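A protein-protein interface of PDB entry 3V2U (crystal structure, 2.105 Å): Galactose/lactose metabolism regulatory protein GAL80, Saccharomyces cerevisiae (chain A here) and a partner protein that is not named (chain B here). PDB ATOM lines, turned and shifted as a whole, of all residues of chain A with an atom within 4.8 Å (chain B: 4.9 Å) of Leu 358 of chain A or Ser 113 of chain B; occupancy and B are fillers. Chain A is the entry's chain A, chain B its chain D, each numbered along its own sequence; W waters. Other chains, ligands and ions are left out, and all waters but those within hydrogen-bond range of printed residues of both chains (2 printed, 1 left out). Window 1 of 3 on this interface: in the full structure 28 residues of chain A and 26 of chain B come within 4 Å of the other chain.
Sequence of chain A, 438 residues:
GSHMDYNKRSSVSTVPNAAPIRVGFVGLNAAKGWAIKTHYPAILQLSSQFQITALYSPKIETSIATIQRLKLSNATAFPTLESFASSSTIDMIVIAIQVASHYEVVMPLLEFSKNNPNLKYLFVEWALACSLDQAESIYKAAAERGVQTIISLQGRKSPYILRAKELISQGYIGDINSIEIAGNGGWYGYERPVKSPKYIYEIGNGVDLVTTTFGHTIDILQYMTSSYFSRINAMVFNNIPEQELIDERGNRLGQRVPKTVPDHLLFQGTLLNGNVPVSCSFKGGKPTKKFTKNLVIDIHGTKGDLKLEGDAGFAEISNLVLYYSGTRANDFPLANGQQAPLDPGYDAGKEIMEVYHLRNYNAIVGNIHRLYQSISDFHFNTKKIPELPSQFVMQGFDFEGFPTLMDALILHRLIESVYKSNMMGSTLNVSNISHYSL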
ATOM      1  N   PRO A 159       9.656  17.483   4.586  1.00  0.00           N
ATOM      2  CA  PRO A 159       8.501  18.388   4.492  1.00  0.00           C
ATOM      3  C   PRO A 159       7.163  17.663   4.224  1.00  0.00           C
ATOM      4  O   PRO A 159       6.101  18.200   4.558  1.00  0.00           O
ATOM      5  CB  PRO A 159       8.864  19.323   3.321  1.00  0.00           C
ATOM      6  CG  PRO A 159       9.965  18.620   2.574  1.00  0.00           C
ATOM      7  CD  PRO A 159      10.717  17.828   3.625  1.00  0.00           C
ATOM      8  N   TYR A 160       7.212  16.473   3.630  1.00  0.00           N
ATOM      9  CA  TYR A 160       5.990  15.761   3.271  1.00  0.00           C
ATOM     10  C   TYR A 160       5.403  15.165   4.532  1.00  0.00           C
ATOM     11  O   TYR A 160       4.188  15.183   4.757  1.00  0.00           O
ATOM     12  CB  TYR A 160       6.292  14.651   2.245  1.00  0.00           C
ATOM     13  CG  TYR A 160       6.705  15.228   0.927  1.00  0.00           C
ATOM     14  CD1 TYR A 160       8.046  15.258   0.545  1.00  0.00           C
ATOM     15  CD2 TYR A 160       5.755  15.795   0.074  1.00  0.00           C
ATOM     16  CE1 TYR A 160       8.422  15.828  -0.670  1.00  0.00           C
ATOM     17  CE2 TYR A 160       6.120  16.365  -1.130  1.00  0.00           C
ATOM     18  CZ  TYR A 160       7.456  16.373  -1.501  1.00  0.00           C
ATOM     19  OH  TYR A 160       7.813  16.940  -2.704  1.00  0.00           O
ATOM     20  N   ASN A 319      11.556  12.226  -2.689  1.00  0.00           N
ATOM     21  CA  ASN A 319      10.587  13.249  -2.995  1.00  0.00           C
ATOM     22  C   ASN A 319       9.245  12.559  -3.200  1.00  0.00           C
ATOM     23  O   ASN A 319       9.133  11.644  -3.997  1.00  0.00           O
ATOM     24  CB  ASN A 319      11.010  14.026  -4.245  1.00  0.00           C
ATOM     25  CG  ASN A 319      10.473  15.432  -4.246  1.00  0.00           C
ATOM     26  OD1 ASN A 319      10.147  15.971  -3.189  1.00  0.00           O
ATOM     27  ND2 ASN A 319      10.368  16.036  -5.427  1.00  0.00           N
ATOM     28  N   TYR A 356       0.244  18.303  -2.411  1.00  0.00           N
ATOM     29  CA  TYR A 356       1.476  18.881  -1.925  1.00  0.00           C
ATOM     30  C   TYR A 356       2.659  18.162  -2.539  1.00  0.00           C
ATOM     31  O   TYR A 356       2.973  17.033  -2.162  1.00  0.00           O
ATOM     32  CB  TYR A 356       1.528  18.799  -0.398  1.00  0.00           C
ATOM     33  CG  TYR A 356       2.707  19.523   0.215  1.00  0.00           C
ATOM     34  CD1 TYR A 356       2.620  20.867   0.568  1.00  0.00           C
ATOM     35  CD2 TYR A 356       3.897  18.854   0.471  1.00  0.00           C
ATOM     36  CE1 TYR A 356       3.718  21.547   1.146  1.00  0.00           C
ATOM     37  CE2 TYR A 356       4.986  19.509   1.048  1.00  0.00           C
ATOM     38  CZ  TYR A 356       4.891  20.850   1.374  1.00  0.00           C
ATOM     39  OH  TYR A 356       5.978  21.477   1.938  1.00  0.00           O
ATOM     40  N   HIS A 357       3.311  18.831  -3.481  1.00  0.00           N
ATOM     41  CA  HIS A 357       4.502  18.302  -4.120  1.00  0.00           C
ATOM     42  C   HIS A 357       5.502  19.410  -4.380  1.00  0.00           C
ATOM     43  O   HIS A 357       5.140  20.472  -4.889  1.00  0.00           O
ATOM     44  CB  HIS A 357       4.179  17.630  -5.464  1.00  0.00           C
ATOM     45  CG  HIS A 357       5.361  16.928  -6.049  1.00  0.00           C
ATOM     46  ND1 HIS A 357       5.888  17.241  -7.286  1.00  0.00           N
ATOM     47  CD2 HIS A 357       6.169  15.980  -5.522  1.00  0.00           C
ATOM     48  CE1 HIS A 357       6.952  16.490  -7.508  1.00  0.00           C
ATOM     49  NE2 HIS A 357       7.141  15.715  -6.456  1.00  0.00           N
ATOM     50  N   LEU A 358       6.764  19.143  -4.060  1.00  0.00           N
ATOM     51  CA  LEU A 358       7.835  20.121  -4.219  1.00  0.00           C
ATOM     52  C   LEU A 358       8.736  19.617  -5.335  1.00  0.00           C
ATOM     53  O   LEU A 358       9.540  18.711  -5.124  1.00  0.00           O
ATOM     54  CB  LEU A 358       8.637  20.240  -2.915  1.00  0.00           C
ATOM     55  CG  LEU A 358       7.819  20.478  -1.645  1.00  0.00           C
ATOM     56  CD1 LEU A 358       8.673  20.212  -0.378  1.00  0.00           C
ATOM     57  CD2 LEU A 358       7.232  21.893  -1.648  1.00  0.00           C
ATOM     58  N   ARG A 359       8.585  20.192  -6.522  1.00  0.00           N
ATOM     59  CA  ARG A 359       9.238  19.659  -7.711  1.00  0.00           C
ATOM     60  C   ARG A 359      10.763  19.650  -7.623  1.00  0.00           C
ATOM     61  O   ARG A 359      11.402  18.667  -7.998  1.00  0.00           O
ATOM     62  CB  ARG A 359       8.782  20.415  -8.962  1.00  0.00           C
ATOM     63  CG  ARG A 359       7.305  20.245  -9.278  1.00  0.00           C
ATOM     64  CD  ARG A 359       6.989  20.710 -10.685  1.00  0.00           C
ATOM     65  NE  ARG A 359       7.534  19.799 -11.686  1.00  0.00           N
ATOM     66  CZ  ARG A 359       7.770  20.137 -12.949  1.00  0.00           C
ATOM     67  NH1 ARG A 359       7.516  21.370 -13.366  1.00  0.00           N
ATOM     68  NH2 ARG A 359       8.270  19.242 -13.795  1.00  0.00           N
ATOM     69  N   ASN A 360      11.353  20.738  -7.141  1.00  0.00           N
ATOM     70  CA  ASN A 360      12.817  20.803  -7.061  1.00  0.00           C
ATOM     71  C   ASN A 360      13.390  20.410  -5.691  1.00  0.00           C
ATOM     72  O   ASN A 360      14.474  20.862  -5.316  1.00  0.00           O
ATOM     73  CB  ASN A 360      13.354  22.182  -7.499  1.00  0.00           C
ATOM     74  CG  ASN A 360      12.922  23.315  -6.568  1.00  0.00           C
ATOM     75  OD1 ASN A 360      11.754  23.408  -6.197  1.00  0.00           O
ATOM     76  ND2 ASN A 360      13.870  24.180  -6.189  1.00  0.00           N
ATOM     77  N   TYR A 361      12.674  19.569  -4.946  1.00  0.00           N
ATOM     78  CA  TYR A 361      13.159  19.172  -3.629  1.00  0.00           C
ATOM     79  C   TYR A 361      14.075  17.952  -3.695  1.00  0.00           C
ATOM     80  O   TYR A 361      13.671  16.875  -4.131  1.00  0.00           O
ATOM     81  CB  TYR A 361      12.017  18.910  -2.648  1.00  0.00           C
ATOM     82  CG  TYR A 361      12.514  18.667  -1.236  1.00  0.00           C
ATOM     83  CD1 TYR A 361      13.145  19.688  -0.518  1.00  0.00           C
ATOM     84  CD2 TYR A 361      12.351  17.432  -0.620  1.00  0.00           C
ATOM     85  CE1 TYR A 361      13.603  19.484   0.771  1.00  0.00           C
ATOM     86  CE2 TYR A 361      12.800  17.215   0.672  1.00  0.00           C
ATOM     87  CZ  TYR A 361      13.429  18.253   1.362  1.00  0.00           C
ATOM     88  OH  TYR A 361      13.891  18.041   2.638  1.00  0.00           O
ATOM     89  N   ARG A 370      17.619  19.453   7.070  1.00  0.00           N
ATOM     90  CA  ARG A 370      16.616  20.003   7.975  1.00  0.00           C
ATOM     91  C   ARG A 370      16.812  19.431   9.374  1.00  0.00           C
ATOM     92  O   ARG A 370      16.475  20.069  10.366  1.00  0.00           O
ATOM     93  CB  ARG A 370      15.193  19.724   7.459  1.00  0.00           C
ATOM     94  CG  ARG A 370      14.818  20.494   6.179  1.00  0.00           C
ATOM     95  CD  ARG A 370      13.659  19.820   5.370  1.00  0.00           C
ATOM     96  NE  ARG A 370      12.371  19.846   6.076  1.00  0.00           N
ATOM     97  CZ  ARG A 370      11.467  20.819   5.978  1.00  0.00           C
ATOM     98  NH1 ARG A 370      11.686  21.868   5.190  1.00  0.00           N
ATOM     99  NH2 ARG A 370      10.325  20.737   6.659  1.00  0.00           N
ATOM    100  N   ASP B 111      15.694  24.713  -0.713  1.00  0.00           N
ATOM    101  CA  ASP B 111      14.548  24.087  -0.053  1.00  0.00           C
ATOM    102  C   ASP B 111      13.350  24.988  -0.265  1.00  0.00           C
ATOM    103  O   ASP B 111      13.215  26.006   0.409  1.00  0.00           O
ATOM    104  CB  ASP B 111      14.795  23.887   1.454  1.00  0.00           C
ATOM    105  CG  ASP B 111      13.656  23.115   2.151  1.00  0.00           C
ATOM    106  OD1 ASP B 111      12.533  23.020   1.598  1.00  0.00           O
ATOM    107  OD2 ASP B 111      13.887  22.600   3.269  1.00  0.00           O
ATOM    108  N   PRO B 112      12.478  24.619  -1.213  1.00  0.00           N
ATOM    109  CA  PRO B 112      11.335  25.465  -1.546  1.00  0.00           C
ATOM    110  C   PRO B 112      10.187  25.283  -0.559  1.00  0.00           C
ATOM    111  O   PRO B 112       9.117  25.799  -0.817  1.00  0.00           O
ATOM    112  CB  PRO B 112      10.904  24.927  -2.926  1.00  0.00           C
ATOM    113  CG  PRO B 112      11.226  23.476  -2.858  1.00  0.00           C
ATOM    114  CD  PRO B 112      12.473  23.353  -1.968  1.00  0.00           C
ATOM    115  N   SER B 113      10.380  24.547   0.532  1.00  0.00           N
ATOM    116  CA  SER B 113       9.249  24.289   1.419  1.00  0.00           C
ATOM    117  C   SER B 113       9.114  25.329   2.539  1.00  0.00           C
ATOM    118  O   SER B 113       8.169  25.271   3.326  1.00  0.00           O
ATOM    119  CB  SER B 113       9.343  22.898   2.034  1.00  0.00           C
ATOM    120  OG  SER B 113      10.414  22.832   2.956  1.00  0.00           O
ATOM    121  N   VAL B 114      10.053  26.264   2.619  1.00  0.00           N
ATOM    122  CA  VAL B 114      10.043  27.234   3.722  1.00  0.00           C
ATOM    123  C   VAL B 114      10.192  28.657   3.205  1.00  0.00           C
ATOM    124  O   VAL B 114      10.746  28.868   2.131  1.00  0.00           O
ATOM    125  CB  VAL B 114      11.170  26.946   4.740  1.00  0.00           C
ATOM    126  CG1 VAL B 114      10.895  25.651   5.483  1.00  0.00           C
ATOM    127  CG2 VAL B 114      12.525  26.902   4.034  1.00  0.00           C
ATOM    128  N   SER B 115       9.668  29.625   3.958  1.00  0.00           N
ATOM    129  CA  SER B 115       9.884  31.027   3.651  1.00  0.00           C
ATOM    130  C   SER B 115      11.242  31.424   4.202  1.00  0.00           C
ATOM    131  O   SER B 115      11.463  31.365   5.407  1.00  0.00           O
ATOM    132  CB  SER B 115       8.804  31.902   4.278  1.00  0.00           C
ATOM    133  OG  SER B 115       9.046  33.263   3.971  1.00  0.00           O
ATOM    134  N   PHE B 259       4.429  33.671   0.527  1.00  0.00           N
ATOM    135  CA  PHE B 259       4.868  32.278   0.430  1.00  0.00           C
ATOM    136  C   PHE B 259       3.953  31.331   1.193  1.00  0.00           C
ATOM    137  O   PHE B 259       3.605  30.266   0.690  1.00  0.00           O
ATOM    138  CB  PHE B 259       6.307  32.080   0.943  1.00  0.00           C
ATOM    139  CG  PHE B 259       6.749  30.641   0.923  1.00  0.00           C
ATOM    140  CD1 PHE B 259       7.288  30.077  -0.232  1.00  0.00           C
ATOM    141  CD2 PHE B 259       6.567  29.834   2.030  1.00  0.00           C
ATOM    142  CE1 PHE B 259       7.669  28.743  -0.266  1.00  0.00           C
ATOM    143  CE2 PHE B 259       6.937  28.494   1.996  1.00  0.00           C
ATOM    144  CZ  PHE B 259       7.493  27.950   0.842  1.00  0.00           C
ATOM    145  N   PRO B 374       2.426  23.311  -4.686  1.00  0.00           N
ATOM    146  CA  PRO B 374       1.407  22.973  -3.686  1.00  0.00           C
ATOM    147  C   PRO B 374       0.164  23.838  -3.870  1.00  0.00           C
ATOM    148  O   PRO B 374       0.262  25.041  -4.179  1.00  0.00           O
ATOM    149  CB  PRO B 374       2.106  23.290  -2.356  1.00  0.00           C
ATOM    150  CG  PRO B 374       3.589  23.061  -2.659  1.00  0.00           C
ATOM    151  CD  PRO B 374       3.741  23.582  -4.081  1.00  0.00           C
HETATM  152  O   HOH W   1       8.234  22.401   5.642  1.00  0.00           O
HETATM  153  O   HOH W   2       5.661  24.046   2.380  1.00  0.00           O
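The side-chain amide nitrogen (ND2) of Asn 319 of chain A is in hydrogen-bond range of a ring nitrogen (NE2) of His 357 of chain A (3.4 Å). ND2 of Asn 319 of chain A is in hydrogen-bond range of O of Leu 358 of chain A, 2.8 Å away. The side-chain hydroxyl of Tyr 160 of chain A lies within hydrogen-bond range of the backbone NH of Leu 358 of chain A (2.8 Å). OG of Ser 113 of chain B is in hydrogen-bond range of OD1 of Asp 111 of chain B, 2.5 Å away.
Printed residues of chain B that touch a printed residue of chain A: Asp 111, Pro 112, Ser 113, Val 114 and Pro 374. Hydrophobic or aromatic side chains of chain B that line the printed part of chain A: Pro 112, Val 114 and Pro 374. Hydrophobic or aromatic side chains of chain A within 4 Å of the printed part of chain B: Pro 159, Tyr 356, Leu 358 and Tyr 361. Among the printed residues, 12 pairs touch across the chains. Among the printed residues, Asp or Glu carboxylates within 4 Å of a Lys or Arg side-chain nitrogen of the other chain: Arg 370 of chain A with Asp 111 of chain B (3.0 Å).
Among the printed residues, pairs that only touch across the chains: Asn 360 of chain A with Pro 112 of chain B (3.4 Å), His 357 of chain A with Pro 374 of chain B (3.5 Å), Tyr 356 of chain A with Ser 113 of chain B (3.7 Å), Leu 358 of chain A with Ser 113 of chain B (3.7 Å), Tyr 361 of chain A with Asp 111 of chain B (3.8 Å), Pro 159 of chain A with Ser 113 of chain B (3.8 Å), Tyr 356 of chain A with Pro 374 of chain B (3.8 Å), Arg 370 of chain A with Val 114 of chain B (3.9 Å), Leu 358 of chain A with Pro 374 of chain B (3.96 Å) and Tyr 361 of chain A with Pro 112 of chain B (3.998 Å).
OD2 of Asp 111 of chain B is in salt-bridge range of NH1 of Arg 370 of chain A. The side-chain hydroxyl (OG) of Ser 113 of chain B is in hydrogen-bond range of the guanidinium group (NH1) of Arg 370 of chain A, at 2.7 Å.
Water W2 bridges OH of Tyr 356 of chain A (2.6 Å) and O of Ser 113 of chain B (2.9 Å). Water W1 bridges the guanidinium group of Arg 370 of chain A and the side-chain hydroxyl of Ser 113 of chain B.
Leu 358 of chain A touches two residues of chain B. Printed residues of chain B within 4 Å of Asn 360 of chain A: Pro 112. Printed residues of chain B within 4 Å of His 357 of chain A: Pro 374 (3.5 Å). Phe 259 of chain B touches none of the printed residues of chain A. The nearest residue of chain B that does not touch Leu 358 of chain A is Pro 112 of chain B (4.1 Å). The nearest printed residue of chain B that does not touch His 357 of chain A is Pro 112 of chain B (7.1 Å).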
